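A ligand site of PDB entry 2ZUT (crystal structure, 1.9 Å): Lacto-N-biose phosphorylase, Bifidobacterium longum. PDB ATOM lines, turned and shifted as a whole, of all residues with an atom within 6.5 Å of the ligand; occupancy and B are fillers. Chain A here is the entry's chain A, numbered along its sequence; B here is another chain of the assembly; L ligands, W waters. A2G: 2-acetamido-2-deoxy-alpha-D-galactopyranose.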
ATOM      1  N   PRO A 161      26.441   1.260  23.408  1.00  0.00           N
ATOM      2  CA  PRO A 161      26.022   1.879  22.152  1.00  0.00           C
ATOM      3  C   PRO A 161      25.625   3.364  22.233  1.00  0.00           C
ATOM      4  O   PRO A 161      25.964   4.153  21.348  1.00  0.00           O
ATOM      5  CB  PRO A 161      24.851   0.996  21.693  1.00  0.00           C
ATOM      6  CG  PRO A 161      25.229  -0.385  22.230  1.00  0.00           C
ATOM      7  CD  PRO A 161      25.825  -0.067  23.609  1.00  0.00           C
ATOM      8  N   VAL A 162      24.895   3.756  23.276  1.00  0.00           N
ATOM      9  CA  VAL A 162      24.445   5.137  23.404  1.00  0.00           C
ATOM     10  C   VAL A 162      25.589   6.118  23.743  1.00  0.00           C
ATOM     11  O   VAL A 162      25.728   7.182  23.105  1.00  0.00           O
ATOM     12  CB  VAL A 162      23.236   5.243  24.355  1.00  0.00           C
ATOM     13  CG1 VAL A 162      22.841   6.667  24.598  1.00  0.00           C
ATOM     14  CG2 VAL A 162      22.043   4.503  23.754  1.00  0.00           C
ATOM     15  N   TYR A 165      27.406   6.473  20.562  1.00  0.00           N
ATOM     16  CA  TYR A 165      26.666   7.410  19.724  1.00  0.00           C
ATOM     17  C   TYR A 165      26.954   8.874  20.122  1.00  0.00           C
ATOM     18  O   TYR A 165      27.296   9.710  19.258  1.00  0.00           O
ATOM     19  CB  TYR A 165      25.148   7.105  19.780  1.00  0.00           C
ATOM     20  CG  TYR A 165      24.346   8.213  19.154  1.00  0.00           C
ATOM     21  CD1 TYR A 165      24.196   8.282  17.759  1.00  0.00           C
ATOM     22  CD2 TYR A 165      23.747   9.187  19.946  1.00  0.00           C
ATOM     23  CE1 TYR A 165      23.473   9.318  17.181  1.00  0.00           C
ATOM     24  CE2 TYR A 165      23.028  10.234  19.375  1.00  0.00           C
ATOM     25  CZ  TYR A 165      22.897  10.282  17.989  1.00  0.00           C
ATOM     26  OH  TYR A 165      22.186  11.328  17.458  1.00  0.00           O
ATOM     27  N   ASN A 166      26.816   9.196  21.402  1.00  0.00           N
ATOM     28  CA  ASN A 166      27.118  10.552  21.873  1.00  0.00           C
ATOM     29  C   ASN A 166      28.575  10.997  21.643  1.00  0.00           C
ATOM     30  O   ASN A 166      28.838  12.150  21.291  1.00  0.00           O
ATOM     31  CB  ASN A 166      26.730  10.689  23.337  1.00  0.00           C
ATOM     32  CG  ASN A 166      25.209  10.680  23.518  1.00  0.00           C
ATOM     33  OD1 ASN A 166      24.703  10.033  24.405  1.00  0.00           O
ATOM     34  ND2 ASN A 166      24.498  11.395  22.648  1.00  0.00           N
ATOM     35  N   GLN A 217      20.002  -2.488  26.020  1.00  0.00           N
ATOM     36  CA  GLN A 217      19.987  -1.458  25.007  1.00  0.00           C
ATOM     37  C   GLN A 217      19.247  -1.908  23.719  1.00  0.00           C
ATOM     38  O   GLN A 217      19.497  -3.011  23.221  1.00  0.00           O
ATOM     39  CB  GLN A 217      21.463  -1.115  24.678  1.00  0.00           C
ATOM     40  CG  GLN A 217      21.682  -0.136  23.497  1.00  0.00           C
ATOM     41  CD  GLN A 217      20.829   1.119  23.583  1.00  0.00           C
ATOM     42  OE1 GLN A 217      20.575   1.637  24.670  1.00  0.00           O
ATOM     43  NE2 GLN A 217      20.388   1.605  22.406  1.00  0.00           N
ATOM     44  N   PHE A 218      18.396  -1.039  23.149  1.00  0.00           N
ATOM     45  CA  PHE A 218      17.757  -1.375  21.872  1.00  0.00           C
ATOM     46  C   PHE A 218      18.822  -1.519  20.778  1.00  0.00           C
ATOM     47  O   PHE A 218      19.846  -0.831  20.811  1.00  0.00           O
ATOM     48  CB  PHE A 218      16.670  -0.362  21.471  1.00  0.00           C
ATOM     49  CG  PHE A 218      17.206   1.024  21.131  1.00  0.00           C
ATOM     50  CD1 PHE A 218      17.777   1.281  19.879  1.00  0.00           C
ATOM     51  CD2 PHE A 218      17.122   2.051  22.067  1.00  0.00           C
ATOM     52  CE1 PHE A 218      18.253   2.565  19.556  1.00  0.00           C
ATOM     53  CE2 PHE A 218      17.574   3.363  21.755  1.00  0.00           C
ATOM     54  CZ  PHE A 218      18.166   3.609  20.511  1.00  0.00           C
ATOM     55  N   LEU A 220      21.408  -1.328  18.252  1.00  0.00           N
ATOM     56  CA  LEU A 220      22.151  -0.146  17.816  1.00  0.00           C
ATOM     57  C   LEU A 220      23.596  -0.582  17.533  1.00  0.00           C
ATOM     58  O   LEU A 220      24.439  -0.652  18.423  1.00  0.00           O
ATOM     59  CB  LEU A 220      22.040   1.012  18.836  1.00  0.00           C
ATOM     60  CG  LEU A 220      22.700   2.353  18.440  1.00  0.00           C
ATOM     61  CD1 LEU A 220      22.152   2.843  17.057  1.00  0.00           C
ATOM     62  CD2 LEU A 220      22.501   3.435  19.512  1.00  0.00           C
ATOM     63  N   PHE A 222      27.062  -0.516  14.892  1.00  0.00           N
ATOM     64  CA  PHE A 222      27.812   0.335  13.967  1.00  0.00           C
ATOM     65  C   PHE A 222      28.738  -0.443  13.043  1.00  0.00           C
ATOM     66  O   PHE A 222      29.109  -1.596  13.329  1.00  0.00           O
ATOM     67  CB  PHE A 222      28.577   1.463  14.714  1.00  0.00           C
ATOM     68  CG  PHE A 222      27.750   2.690  14.990  1.00  0.00           C
ATOM     69  CD1 PHE A 222      26.486   2.597  15.513  1.00  0.00           C
ATOM     70  CD2 PHE A 222      28.269   3.964  14.732  1.00  0.00           C
ATOM     71  CE1 PHE A 222      25.719   3.744  15.760  1.00  0.00           C
ATOM     72  CE2 PHE A 222      27.525   5.119  14.981  1.00  0.00           C
ATOM     73  CZ  PHE A 222      26.232   5.004  15.485  1.00  0.00           C
ATOM     74  N   GLU A 228      26.085   4.185  11.670  1.00  0.00           N
ATOM     75  CA  GLU A 228      25.064   3.205  12.072  1.00  0.00           C
ATOM     76  C   GLU A 228      24.932   2.127  11.015  1.00  0.00           C
ATOM     77  O   GLU A 228      24.889   2.414   9.795  1.00  0.00           O
ATOM     78  CB  GLU A 228      23.745   3.874  12.321  1.00  0.00           C
ATOM     79  CG  GLU A 228      22.745   3.026  13.112  1.00  0.00           C
ATOM     80  CD  GLU A 228      21.409   3.663  13.077  1.00  0.00           C
ATOM     81  OE1 GLU A 228      21.086   4.362  14.056  1.00  0.00           O
ATOM     82  OE2 GLU A 228      20.694   3.532  12.017  1.00  0.00           O
ATOM     83  N   VAL A 231      19.723  -0.615  13.246  1.00  0.00           N
ATOM     84  CA  VAL A 231      18.979  -0.023  14.364  1.00  0.00           C
ATOM     85  C   VAL A 231      17.548  -0.517  14.429  1.00  0.00           C
ATOM     86  O   VAL A 231      16.875  -0.654  13.370  1.00  0.00           O
ATOM     87  CB  VAL A 231      18.969   1.545  14.311  1.00  0.00           C
ATOM     88  CG1 VAL A 231      18.147   2.100  13.094  1.00  0.00           C
ATOM     89  CG2 VAL A 231      18.485   2.153  15.641  1.00  0.00           C
ATOM     90  N   TRP A 233      14.474   0.475  17.340  1.00  0.00           N
ATOM     91  CA  TRP A 233      14.176   1.057  18.637  1.00  0.00           C
ATOM     92  C   TRP A 233      13.519   0.013  19.559  1.00  0.00           C
ATOM     93  O   TRP A 233      13.554   0.133  20.774  1.00  0.00           O
ATOM     94  CB  TRP A 233      13.324   2.328  18.475  1.00  0.00           C
ATOM     95  CG  TRP A 233      13.179   3.110  19.749  1.00  0.00           C
ATOM     96  CD1 TRP A 233      14.177   3.633  20.484  1.00  0.00           C
ATOM     97  CD2 TRP A 233      11.956   3.446  20.418  1.00  0.00           C
ATOM     98  NE1 TRP A 233      13.669   4.259  21.594  1.00  0.00           N
ATOM     99  CE2 TRP A 233      12.305   4.154  21.585  1.00  0.00           C
ATOM    100  CE3 TRP A 233      10.599   3.208  20.151  1.00  0.00           C
ATOM    101  CZ2 TRP A 233      11.346   4.641  22.499  1.00  0.00           C
ATOM    102  CZ3 TRP A 233       9.631   3.697  21.066  1.00  0.00           C
ATOM    103  CH2 TRP A 233      10.008   4.406  22.215  1.00  0.00           C
ATOM    104  N   PHE A 310      13.214   6.287  31.737  1.00  0.00           N
ATOM    105  CA  PHE A 310      13.263   6.911  30.417  1.00  0.00           C
ATOM    106  C   PHE A 310      12.763   5.888  29.394  1.00  0.00           C
ATOM    107  O   PHE A 310      13.257   4.747  29.326  1.00  0.00           O
ATOM    108  CB  PHE A 310      14.697   7.319  30.073  1.00  0.00           C
ATOM    109  CG  PHE A 310      14.885   7.820  28.648  1.00  0.00           C
ATOM    110  CD1 PHE A 310      14.181   8.925  28.187  1.00  0.00           C
ATOM    111  CD2 PHE A 310      15.777   7.177  27.777  1.00  0.00           C
ATOM    112  CE1 PHE A 310      14.347   9.398  26.880  1.00  0.00           C
ATOM    113  CE2 PHE A 310      15.982   7.658  26.447  1.00  0.00           C
ATOM    114  CZ  PHE A 310      15.255   8.774  26.011  1.00  0.00           C
ATOM    115  N   LEU A 311      11.749   6.292  28.634  1.00  0.00           N
ATOM    116  CA  LEU A 311      11.225   5.449  27.566  1.00  0.00           C
ATOM    117  C   LEU A 311      12.180   5.476  26.379  1.00  0.00           C
ATOM    118  O   LEU A 311      12.008   6.252  25.423  1.00  0.00           O
ATOM    119  CB  LEU A 311       9.838   5.968  27.136  1.00  0.00           C
ATOM    120  CG  LEU A 311       9.117   5.059  26.137  1.00  0.00           C
ATOM    121  CD1 LEU A 311       8.699   3.759  26.829  1.00  0.00           C
ATOM    122  CD2 LEU A 311       7.913   5.729  25.443  1.00  0.00           C
ATOM    123  N   GLY A 312      13.230   4.656  26.427  1.00  0.00           N
ATOM    124  CA  GLY A 312      14.251   4.710  25.417  1.00  0.00           C
ATOM    125  C   GLY A 312      15.518   4.084  25.925  1.00  0.00           C
ATOM    126  O   GLY A 312      15.529   3.556  27.048  1.00  0.00           O
ATOM    127  N   ASP A 313      16.550   4.116  25.076  1.00  0.00           N
ATOM    128  CA  ASP A 313      17.854   3.490  25.330  1.00  0.00           C
ATOM    129  C   ASP A 313      17.714   2.079  25.919  1.00  0.00           C
ATOM    130  O   ASP A 313      17.165   1.189  25.250  1.00  0.00           O
ATOM    131  CB  ASP A 313      18.756   4.408  26.193  1.00  0.00           C
ATOM    132  CG  ASP A 313      19.017   5.781  25.527  1.00  0.00           C
ATOM    133  OD1 ASP A 313      18.651   5.948  24.337  1.00  0.00           O
ATOM    134  OD2 ASP A 313      19.584   6.684  26.219  1.00  0.00           O
ATOM    135  N   GLN A 314      18.194   1.863  27.152  1.00  0.00           N
ATOM    136  CA  GLN A 314      18.101   0.518  27.746  1.00  0.00           C
ATOM    137  C   GLN A 314      16.716   0.125  28.252  1.00  0.00           C
ATOM    138  O   GLN A 314      16.556  -0.280  29.426  1.00  0.00           O
ATOM    139  CB  GLN A 314      19.185   0.286  28.797  1.00  0.00           C
ATOM    140  CG  GLN A 314      20.577   0.354  28.214  1.00  0.00           C
ATOM    141  CD  GLN A 314      21.155   1.735  28.350  1.00  0.00           C
ATOM    142  OE1 GLN A 314      20.477   2.667  28.780  1.00  0.00           O
ATOM    143  NE2 GLN A 314      22.428   1.868  28.018  1.00  0.00           N
ATOM    144  N   TRP A 315      15.712   0.205  27.382  1.00  0.00           N
ATOM    145  CA  TRP A 315      14.355  -0.104  27.788  1.00  0.00           C
ATOM    146  C   TRP A 315      13.810  -1.491  27.337  1.00  0.00           C
ATOM    147  O   TRP A 315      12.672  -1.817  27.613  1.00  0.00           O
ATOM    148  CB  TRP A 315      13.408   1.013  27.348  1.00  0.00           C
ATOM    149  CG  TRP A 315      13.085   0.958  25.858  1.00  0.00           C
ATOM    150  CD1 TRP A 315      13.959   1.105  24.803  1.00  0.00           C
ATOM    151  CD2 TRP A 315      11.798   0.731  25.282  1.00  0.00           C
ATOM    152  NE1 TRP A 315      13.271   1.013  23.589  1.00  0.00           N
ATOM    153  CE2 TRP A 315      11.959   0.756  23.865  1.00  0.00           C
ATOM    154  CE3 TRP A 315      10.523   0.518  25.824  1.00  0.00           C
ATOM    155  CZ2 TRP A 315      10.879   0.584  22.988  1.00  0.00           C
ATOM    156  CZ3 TRP A 315       9.437   0.325  24.943  1.00  0.00           C
ATOM    157  CH2 TRP A 315       9.636   0.378  23.531  1.00  0.00           C
ATOM    158  N   GLY A 335       9.860  10.621  28.584  1.00  0.00           N
ATOM    159  CA  GLY A 335      10.323  10.265  27.245  1.00  0.00           C
ATOM    160  C   GLY A 335      10.551  11.469  26.361  1.00  0.00           C
ATOM    161  O   GLY A 335      10.219  12.588  26.750  1.00  0.00           O
ATOM    162  N   SER A 336      11.142  11.243  25.191  1.00  0.00           N
ATOM    163  CA  SER A 336      11.462  12.310  24.238  1.00  0.00           C
ATOM    164  C   SER A 336      10.236  12.668  23.419  1.00  0.00           C
ATOM    165  O   SER A 336       9.623  11.789  22.829  1.00  0.00           O
ATOM    166  CB  SER A 336      12.553  11.902  23.229  1.00  0.00           C
ATOM    167  OG  SER A 336      13.626  11.233  23.852  1.00  0.00           O
ATOM    168  N   ALA A 459      13.822   3.795  13.524  1.00  0.00           N
ATOM    169  CA  ALA A 459      14.471   4.662  14.521  1.00  0.00           C
ATOM    170  C   ALA A 459      13.431   5.623  15.085  1.00  0.00           C
ATOM    171  O   ALA A 459      12.583   6.151  14.337  1.00  0.00           O
ATOM    172  CB  ALA A 459      15.634   5.450  13.911  1.00  0.00           C
ATOM    173  N   HIS A 460      13.483   5.819  16.395  1.00  0.00           N
ATOM    174  CA  HIS A 460      12.607   6.736  17.125  1.00  0.00           C
ATOM    175  C   HIS A 460      12.482   8.125  16.496  1.00  0.00           C
ATOM    176  O   HIS A 460      13.479   8.829  16.300  1.00  0.00           O
ATOM    177  CB  HIS A 460      13.055   6.851  18.600  1.00  0.00           C
ATOM    178  CG  HIS A 460      12.073   7.570  19.468  1.00  0.00           C
ATOM    179  ND1 HIS A 460      12.097   8.929  19.632  1.00  0.00           N
ATOM    180  CD2 HIS A 460      11.001   7.117  20.168  1.00  0.00           C
ATOM    181  CE1 HIS A 460      11.118   9.294  20.431  1.00  0.00           C
ATOM    182  NE2 HIS A 460      10.429   8.223  20.763  1.00  0.00           N
ATOM    183  N   LEU A 462      12.073   9.121  13.562  1.00  0.00           N
ATOM    184  CA  LEU A 462      12.784   9.371  12.285  1.00  0.00           C
ATOM    185  C   LEU A 462      12.106   8.674  11.088  1.00  0.00           C
ATOM    186  O   LEU A 462      12.648   7.729  10.528  1.00  0.00           O
ATOM    187  CB  LEU A 462      14.257   8.952  12.393  1.00  0.00           C
ATOM    188  CG  LEU A 462      15.068   9.936  13.256  1.00  0.00           C
ATOM    189  CD1 LEU A 462      16.504   9.418  13.481  1.00  0.00           C
ATOM    190  CD2 LEU A 462      15.103  11.324  12.637  1.00  0.00           C
ATOM    191  N   SER B 612      20.182   8.150  11.571  1.00  0.00           N
ATOM    192  CA  SER B 612      19.737   6.879  12.159  1.00  0.00           C
ATOM    193  C   SER B 612      18.474   6.345  11.466  1.00  0.00           C
ATOM    194  O   SER B 612      17.525   7.090  11.237  1.00  0.00           O
ATOM    195  CB  SER B 612      19.448   7.043  13.663  1.00  0.00           C
ATOM    196  OG  SER B 612      18.929   5.804  14.168  1.00  0.00           O
HETATM  197  O5  A2G L   1      18.492   6.920  19.305  1.00  0.00           O
HETATM  198  C1  A2G L   1      17.260   7.368  19.877  1.00  0.00           C
HETATM  199  O1  A2G L   1      16.947   8.684  19.411  1.00  0.00           O
HETATM  200  C2  A2G L   1      17.418   7.439  21.409  1.00  0.00           C
HETATM  201  N2  A2G L   1      16.201   7.943  22.039  1.00  0.00           N
HETATM  202  C3  A2G L   1      18.618   8.322  21.765  1.00  0.00           C
HETATM  203  O3  A2G L   1      18.799   8.284  23.177  1.00  0.00           O
HETATM  204  C4  A2G L   1      19.890   7.787  21.127  1.00  0.00           C
HETATM  205  O4  A2G L   1      20.173   6.479  21.684  1.00  0.00           O
HETATM  206  C5  A2G L   1      19.667   7.681  19.621  1.00  0.00           C
HETATM  207  C6  A2G L   1      20.847   7.062  18.889  1.00  0.00           C
HETATM  208  O6  A2G L   1      20.566   7.168  17.478  1.00  0.00           O
HETATM  209  C7  A2G L   1      15.325   7.122  22.653  1.00  0.00           C
HETATM  210  O7  A2G L   1      15.578   5.964  22.930  1.00  0.00           O
HETATM  211  C8  A2G L   1      13.967   7.677  22.885  1.00  0.00           C
HETATM  212  O   HOH W   1      17.945  11.462  19.575  1.00  0.00           O
HETATM  213  O   HOH W   2      15.429  10.857  21.687  1.00  0.00           O
HETATM  214  O   HOH W   3      21.613  10.258  23.146  1.00  0.00           O
HETATM  215  O   HOH W   4      16.116   8.412  16.931  1.00  0.00           O
HETATM  216  O   HOH W   5      22.381   6.019  15.643  1.00  0.00           O
HETATM  217  O   HOH W   6      20.355   9.617  16.103  1.00  0.00           O
HETATM  218  O   HOH W   7      17.822   6.294  16.574  1.00  0.00           O
HETATM  219  O   HOH W   8      18.261  10.693  24.360  1.00  0.00           O
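Residues that only touch the ligand: Gly 312 (3.1 Å), Val 162 (3.4 Å), Phe 218 (3.5 Å), Leu 311 (3.5 Å), Phe 310 (3.6 Å), Tyr 165 (3.6 Å), Ser 336 (3.7 Å), His 460 (3.9 Å) and Ser 612 of chain B (3.9 Å). Hydrophobic or aromatic side chains within 4 Å of the ligand: Val 162, Tyr 165, Phe 218, Trp 233, Phe 310 and His 460. The nearest printed residue that does not touch the ligand is Leu 220 (4.03 Å).
OD1 of Asn 166 sits close to O of Val 162 (3.3 Å). N of Phe 218 sits close to O of Asp 313, 3.3 Å away. The side-chain carboxylate (OE1) of Glu 228 sits at hydrogen-bond distance from the side-chain hydroxyl (OG) of Ser 612 of chain B, at 2.6 Å. The backbone carbonyl oxygen (O) of Trp 233 lies within hydrogen-bond range of the indole nitrogen (NE1) of Trp 315 (3.0 Å). The side-chain amide oxygen of Gln 217 lies close to the backbone carbonyl oxygen of Asp 313, 3.5 Å away.
The side-chain carboxylate (OD1) of Asp 313 is in hydrogen-bond range of an oxygen (O3) of the ligand (2.6 Å). NE1 of Trp 233 lies within hydrogen-bond range of O7 of the ligand (2.9 Å). The backbone NH (N) of Asp 313 is in hydrogen-bond range of an oxygen (O7) of the ligand (3.0 Å).
Water W4 lies within hydrogen-bond range of O1 of the ligand (2.6 Å) and O of His 460 (2.7 Å). Water W6 bridges O6 of the ligand (2.8 Å) and OH of Tyr 165 (2.8 Å). Water W5 lies within hydrogen-bond range of OE1 of Glu 228 (2.6 Å) and O6 of the ligand (2.8 Å). Water W7 bridges the side-chain hydroxyl of Ser 612 of chain B and an oxygen (O5) of the ligand. Water W2 lies within hydrogen-bond range of OG of Ser 336 (2.8 Å) and N2 of the ligand (3.0 Å). Water W3 bridges ND2 of Asn 166 and O3 of the ligand.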
